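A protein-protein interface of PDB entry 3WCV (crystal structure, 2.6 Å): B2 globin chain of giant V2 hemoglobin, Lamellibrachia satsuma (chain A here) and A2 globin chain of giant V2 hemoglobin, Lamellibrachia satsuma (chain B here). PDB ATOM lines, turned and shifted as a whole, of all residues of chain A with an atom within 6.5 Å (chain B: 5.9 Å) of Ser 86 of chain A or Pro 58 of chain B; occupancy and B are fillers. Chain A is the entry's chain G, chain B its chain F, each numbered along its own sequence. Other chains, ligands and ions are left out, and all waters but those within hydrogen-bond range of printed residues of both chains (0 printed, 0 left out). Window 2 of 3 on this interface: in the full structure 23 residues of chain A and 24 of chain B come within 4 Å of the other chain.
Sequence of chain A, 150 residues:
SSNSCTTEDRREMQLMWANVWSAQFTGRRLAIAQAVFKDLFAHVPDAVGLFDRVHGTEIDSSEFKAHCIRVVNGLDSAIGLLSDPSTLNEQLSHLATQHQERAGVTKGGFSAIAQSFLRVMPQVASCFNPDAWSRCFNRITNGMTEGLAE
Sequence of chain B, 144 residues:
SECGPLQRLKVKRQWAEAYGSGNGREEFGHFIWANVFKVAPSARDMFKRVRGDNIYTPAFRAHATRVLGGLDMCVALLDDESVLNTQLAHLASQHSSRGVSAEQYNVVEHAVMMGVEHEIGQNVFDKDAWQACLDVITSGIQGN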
ATOM      1  N   LEU A  81     -32.444   3.269  -1.641  1.00  0.00           N
ATOM      2  CA  LEU A  81     -32.308   4.728  -1.564  1.00  0.00           C
ATOM      3  C   LEU A  81     -33.449   5.491  -0.872  1.00  0.00           C
ATOM      4  O   LEU A  81     -33.428   6.714  -0.829  1.00  0.00           O
ATOM      5  CB  LEU A  81     -32.045   5.315  -2.956  1.00  0.00           C
ATOM      6  CG  LEU A  81     -30.681   4.950  -3.540  1.00  0.00           C
ATOM      7  CD1 LEU A  81     -30.582   5.480  -4.959  1.00  0.00           C
ATOM      8  CD2 LEU A  81     -29.581   5.517  -2.676  1.00  0.00           C
ATOM      9  N   ASP A  84     -31.938   7.711   1.628  1.00  0.00           N
ATOM     10  CA  ASP A  84     -31.297   8.955   1.221  1.00  0.00           C
ATOM     11  C   ASP A  84     -32.050   9.526   0.021  1.00  0.00           C
ATOM     12  O   ASP A  84     -31.650   9.349  -1.129  1.00  0.00           O
ATOM     13  CB  ASP A  84     -29.830   8.701   0.864  1.00  0.00           C
ATOM     14  CG  ASP A  84     -29.117   9.959   0.432  1.00  0.00           C
ATOM     15  OD1 ASP A  84     -29.140  10.954   1.182  1.00  0.00           O
ATOM     16  OD2 ASP A  84     -28.530   9.957  -0.668  1.00  0.00           O
ATOM     17  N   PRO A  85     -33.173  10.203   0.278  1.00  0.00           N
ATOM     18  CA  PRO A  85     -34.006  10.806  -0.770  1.00  0.00           C
ATOM     19  C   PRO A  85     -33.281  11.660  -1.827  1.00  0.00           C
ATOM     20  O   PRO A  85     -33.607  11.579  -3.003  1.00  0.00           O
ATOM     21  CB  PRO A  85     -35.031  11.604   0.034  1.00  0.00           C
ATOM     22  CG  PRO A  85     -35.207  10.755   1.268  1.00  0.00           C
ATOM     23  CD  PRO A  85     -33.782  10.392   1.609  1.00  0.00           C
ATOM     24  N   SER A  86     -32.310  12.472  -1.423  1.00  0.00           N
ATOM     25  CA  SER A  86     -31.589  13.307  -2.388  1.00  0.00           C
ATOM     26  C   SER A  86     -31.119  12.436  -3.540  1.00  0.00           C
ATOM     27  O   SER A  86     -31.424  12.721  -4.702  1.00  0.00           O
ATOM     28  CB  SER A  86     -30.382  13.991  -1.741  1.00  0.00           C
ATOM     29  OG  SER A  86     -29.328  13.071  -1.502  1.00  0.00           O
ATOM     30  N   THR A  87     -30.385  11.371  -3.208  1.00  0.00           N
ATOM     31  CA  THR A  87     -29.864  10.431  -4.202  1.00  0.00           C
ATOM     32  C   THR A  87     -30.975   9.656  -4.890  1.00  0.00           C
ATOM     33  O   THR A  87     -30.837   9.294  -6.048  1.00  0.00           O
ATOM     34  CB  THR A  87     -28.903   9.406  -3.575  1.00  0.00           C
ATOM     35  OG1 THR A  87     -27.787  10.093  -2.993  1.00  0.00           O
ATOM     36  CG2 THR A  87     -28.387   8.447  -4.630  1.00  0.00           C
ATOM     37  N   LEU A  88     -32.063   9.394  -4.169  1.00  0.00           N
ATOM     38  CA  LEU A  88     -33.201   8.658  -4.717  1.00  0.00           C
ATOM     39  C   LEU A  88     -33.750   9.398  -5.919  1.00  0.00           C
ATOM     40  O   LEU A  88     -33.943   8.835  -7.002  1.00  0.00           O
ATOM     41  CB  LEU A  88     -34.316   8.529  -3.677  1.00  0.00           C
ATOM     42  CG  LEU A  88     -35.650   7.927  -4.171  1.00  0.00           C
ATOM     43  CD1 LEU A  88     -35.382   6.498  -4.641  1.00  0.00           C
ATOM     44  CD2 LEU A  88     -36.724   7.944  -3.046  1.00  0.00           C
ATOM     45  N   ASN A  89     -34.002  10.682  -5.714  1.00  0.00           N
ATOM     46  CA  ASN A  89     -34.545  11.513  -6.766  1.00  0.00           C
ATOM     47  C   ASN A  89     -33.731  11.400  -8.046  1.00  0.00           C
ATOM     48  O   ASN A  89     -34.298  11.302  -9.123  1.00  0.00           O
ATOM     49  CB  ASN A  89     -34.651  12.958  -6.283  1.00  0.00           C
ATOM     50  CG  ASN A  89     -35.754  13.143  -5.249  1.00  0.00           C
ATOM     51  OD1 ASN A  89     -36.803  12.494  -5.319  1.00  0.00           O
ATOM     52  ND2 ASN A  89     -35.531  14.047  -4.294  1.00  0.00           N
ATOM     53  N   GLU A  90     -32.406  11.385  -7.936  1.00  0.00           N
ATOM     54  CA  GLU A  90     -31.563  11.254  -9.128  1.00  0.00           C
ATOM     55  C   GLU A  90     -31.768   9.894  -9.817  1.00  0.00           C
ATOM     56  O   GLU A  90     -31.934   9.821 -11.044  1.00  0.00           O
ATOM     57  CB  GLU A  90     -30.083  11.442  -8.766  1.00  0.00           C
ATOM     58  CG  GLU A  90     -29.741  12.860  -8.341  1.00  0.00           C
ATOM     59  CD  GLU A  90     -30.212  13.902  -9.353  1.00  0.00           C
ATOM     60  OE1 GLU A  90     -29.664  13.928 -10.473  1.00  0.00           O
ATOM     61  OE2 GLU A  90     -31.133  14.684  -9.031  1.00  0.00           O
ATOM     62  N   GLN A  91     -31.767   8.830  -9.020  1.00  0.00           N
ATOM     63  CA  GLN A  91     -31.955   7.476  -9.519  1.00  0.00           C
ATOM     64  C   GLN A  91     -33.312   7.276 -10.178  1.00  0.00           C
ATOM     65  O   GLN A  91     -33.412   6.568 -11.177  1.00  0.00           O
ATOM     66  CB  GLN A  91     -31.793   6.476  -8.371  1.00  0.00           C
ATOM     67  CG  GLN A  91     -32.079   5.038  -8.733  1.00  0.00           C
ATOM     68  CD  GLN A  91     -31.069   4.477  -9.707  1.00  0.00           C
ATOM     69  OE1 GLN A  91     -30.023   5.082  -9.961  1.00  0.00           O
ATOM     70  NE2 GLN A  91     -31.365   3.301 -10.247  1.00  0.00           N
ATOM     71  N   TYR B  56     -19.375  13.296  -4.195  1.00  0.00           N
ATOM     72  CA  TYR B  56     -20.159  13.521  -2.985  1.00  0.00           C
ATOM     73  C   TYR B  56     -21.559  13.990  -3.376  1.00  0.00           C
ATOM     74  O   TYR B  56     -22.402  14.230  -2.515  1.00  0.00           O
ATOM     75  CB  TYR B  56     -19.503  14.595  -2.102  1.00  0.00           C
ATOM     76  CG  TYR B  56     -18.093  14.277  -1.677  1.00  0.00           C
ATOM     77  CD1 TYR B  56     -17.844  13.527  -0.535  1.00  0.00           C
ATOM     78  CD2 TYR B  56     -16.997  14.702  -2.436  1.00  0.00           C
ATOM     79  CE1 TYR B  56     -16.541  13.203  -0.150  1.00  0.00           C
ATOM     80  CE2 TYR B  56     -15.691  14.381  -2.061  1.00  0.00           C
ATOM     81  CZ  TYR B  56     -15.475  13.635  -0.920  1.00  0.00           C
ATOM     82  OH  TYR B  56     -14.189  13.326  -0.539  1.00  0.00           O
ATOM     83  N   THR B  57     -21.814  14.133  -4.668  1.00  0.00           N
ATOM     84  CA  THR B  57     -23.128  14.599  -5.101  1.00  0.00           C
ATOM     85  C   THR B  57     -24.154  13.490  -5.305  1.00  0.00           C
ATOM     86  O   THR B  57     -23.813  12.362  -5.632  1.00  0.00           O
ATOM     87  CB  THR B  57     -23.024  15.431  -6.401  1.00  0.00           C
ATOM     88  OG1 THR B  57     -22.389  14.656  -7.422  1.00  0.00           O
ATOM     89  CG2 THR B  57     -22.216  16.685  -6.156  1.00  0.00           C
ATOM     90  N   PRO B  58     -25.430  13.809  -5.090  1.00  0.00           N
ATOM     91  CA  PRO B  58     -26.489  12.818  -5.259  1.00  0.00           C
ATOM     92  C   PRO B  58     -26.428  12.232  -6.652  1.00  0.00           C
ATOM     93  O   PRO B  58     -26.624  11.025  -6.834  1.00  0.00           O
ATOM     94  CB  PRO B  58     -27.757  13.625  -5.006  1.00  0.00           C
ATOM     95  CG  PRO B  58     -27.311  14.579  -3.932  1.00  0.00           C
ATOM     96  CD  PRO B  58     -25.958  15.041  -4.479  1.00  0.00           C
ATOM     97  N   ALA B  59     -26.135  13.092  -7.622  1.00  0.00           N
ATOM     98  CA  ALA B  59     -26.033  12.688  -9.018  1.00  0.00           C
ATOM     99  C   ALA B  59     -25.033  11.552  -9.168  1.00  0.00           C
ATOM    100  O   ALA B  59     -25.368  10.473  -9.695  1.00  0.00           O
ATOM    101  CB  ALA B  59     -25.595  13.863  -9.858  1.00  0.00           C
ATOM    102  N   PHE B  60     -23.807  11.790  -8.693  1.00  0.00           N
ATOM    103  CA  PHE B  60     -22.792  10.758  -8.795  1.00  0.00           C
ATOM    104  C   PHE B  60     -23.107   9.521  -7.980  1.00  0.00           C
ATOM    105  O   PHE B  60     -22.863   8.392  -8.424  1.00  0.00           O
ATOM    106  CB  PHE B  60     -21.418  11.230  -8.364  1.00  0.00           C
ATOM    107  CG  PHE B  60     -20.341  10.238  -8.709  1.00  0.00           C
ATOM    108  CD1 PHE B  60     -19.846  10.161 -10.010  1.00  0.00           C
ATOM    109  CD2 PHE B  60     -19.893   9.316  -7.760  1.00  0.00           C
ATOM    110  CE1 PHE B  60     -18.925   9.180 -10.362  1.00  0.00           C
ATOM    111  CE2 PHE B  60     -18.969   8.324  -8.103  1.00  0.00           C
ATOM    112  CZ  PHE B  60     -18.487   8.255  -9.403  1.00  0.00           C
ATOM    113  N   ARG B  61     -23.637   9.735  -6.781  1.00  0.00           N
ATOM    114  CA  ARG B  61     -23.966   8.618  -5.909  1.00  0.00           C
ATOM    115  C   ARG B  61     -24.991   7.722  -6.602  1.00  0.00           C
ATOM    116  O   ARG B  61     -24.912   6.489  -6.508  1.00  0.00           O
ATOM    117  CB  ARG B  61     -24.483   9.135  -4.554  1.00  0.00           C
ATOM    118  CG  ARG B  61     -23.400   9.818  -3.716  1.00  0.00           C
ATOM    119  CD  ARG B  61     -23.968  10.321  -2.410  1.00  0.00           C
ATOM    120  NE  ARG B  61     -23.058  11.208  -1.674  1.00  0.00           N
ATOM    121  CZ  ARG B  61     -21.945  10.813  -1.047  1.00  0.00           C
ATOM    122  NH1 ARG B  61     -21.192  11.696  -0.393  1.00  0.00           N
ATOM    123  NH2 ARG B  61     -21.579   9.533  -1.076  1.00  0.00           N
ATOM    124  N   ALA B  62     -25.925   8.346  -7.322  1.00  0.00           N
ATOM    125  CA  ALA B  62     -26.943   7.580  -8.026  1.00  0.00           C
ATOM    126  C   ALA B  62     -26.258   6.748  -9.098  1.00  0.00           C
ATOM    127  O   ALA B  62     -26.637   5.598  -9.327  1.00  0.00           O
ATOM    128  CB  ALA B  62     -27.974   8.483  -8.643  1.00  0.00           C
ATOM    129  N   HIS B  63     -25.244   7.325  -9.748  1.00  0.00           N
ATOM    130  CA  HIS B  63     -24.513   6.590 -10.770  1.00  0.00           C
ATOM    131  C   HIS B  63     -23.816   5.361 -10.137  1.00  0.00           C
ATOM    132  O   HIS B  63     -23.927   4.244 -10.645  1.00  0.00           O
ATOM    133  CB  HIS B  63     -23.481   7.499 -11.468  1.00  0.00           C
ATOM    134  CG  HIS B  63     -22.485   6.744 -12.292  1.00  0.00           C
ATOM    135  ND1 HIS B  63     -22.841   6.008 -13.403  1.00  0.00           N
ATOM    136  CD2 HIS B  63     -21.162   6.519 -12.100  1.00  0.00           C
ATOM    137  CE1 HIS B  63     -21.784   5.356 -13.854  1.00  0.00           C
ATOM    138  NE2 HIS B  63     -20.751   5.647 -13.081  1.00  0.00           N
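O of Ala 62 of chain B lies close to OE1 of Gln 91 of chain A, at 3.5 Å.
The side-chain carboxylate of Asp 84 of chain A lies within hydrogen-bond range of the side-chain hydroxyl of Thr 87 of chain A, 2.4 Å away. The side-chain carboxylate (OD2) of Asp 84 of chain A lies within hydrogen-bond range of the side-chain hydroxyl (OG) of Ser 86 of chain A, at 3.3 Å. The backbone carbonyl oxygen (O) of Tyr 56 of chain B sits at hydrogen-bond distance from the guanidinium group (NE) of Arg 61 of chain B.
Pro 58 of chain B touches Ser 86 of chain A (CG to OG, 3.5 Å). Thr 87 of chain A touches Pro 58 of chain B (OG1 to CA, 3.8 Å). Thr 87 of chain A touches Arg 61 of chain B (OG1 to CB, 3.8 Å). Thr 87 of chain A touches Ala 62 of chain B (CG2 to N, 3.6 Å). Glu 90 of chain A touches Pro 58 of chain B (CG to C, 3.8 Å). Glu 90 of chain A touches Ala 59 of chain B (CG to N, 3.7 Å). Glu 90 of chain A touches Ala 62 of chain B (CB to CB, 3.6 Å).
Ser 86 of chain A touches one residue of chain B. Pro 58 of chain B touches just these residues of chain A: Ser 86 (3.5 Å), Thr 87 (3.8 Å) and Glu 90 (3.8 Å). Of the printed residues of chain A, Ala 59 of chain B touches Glu 90. Of the printed residues of chain A, Arg 61 of chain B touches Thr 87. The nearest printed residue of chain B that does not touch Gln 91 of chain A is His 63 of chain B (5.3 Å).
Among the printed residues, 8 pairs touch across the chains. Among the printed residues, no Asp or Glu carboxylate lies within 4 Å of a Lys or Arg side-chain nitrogen of the other chain.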
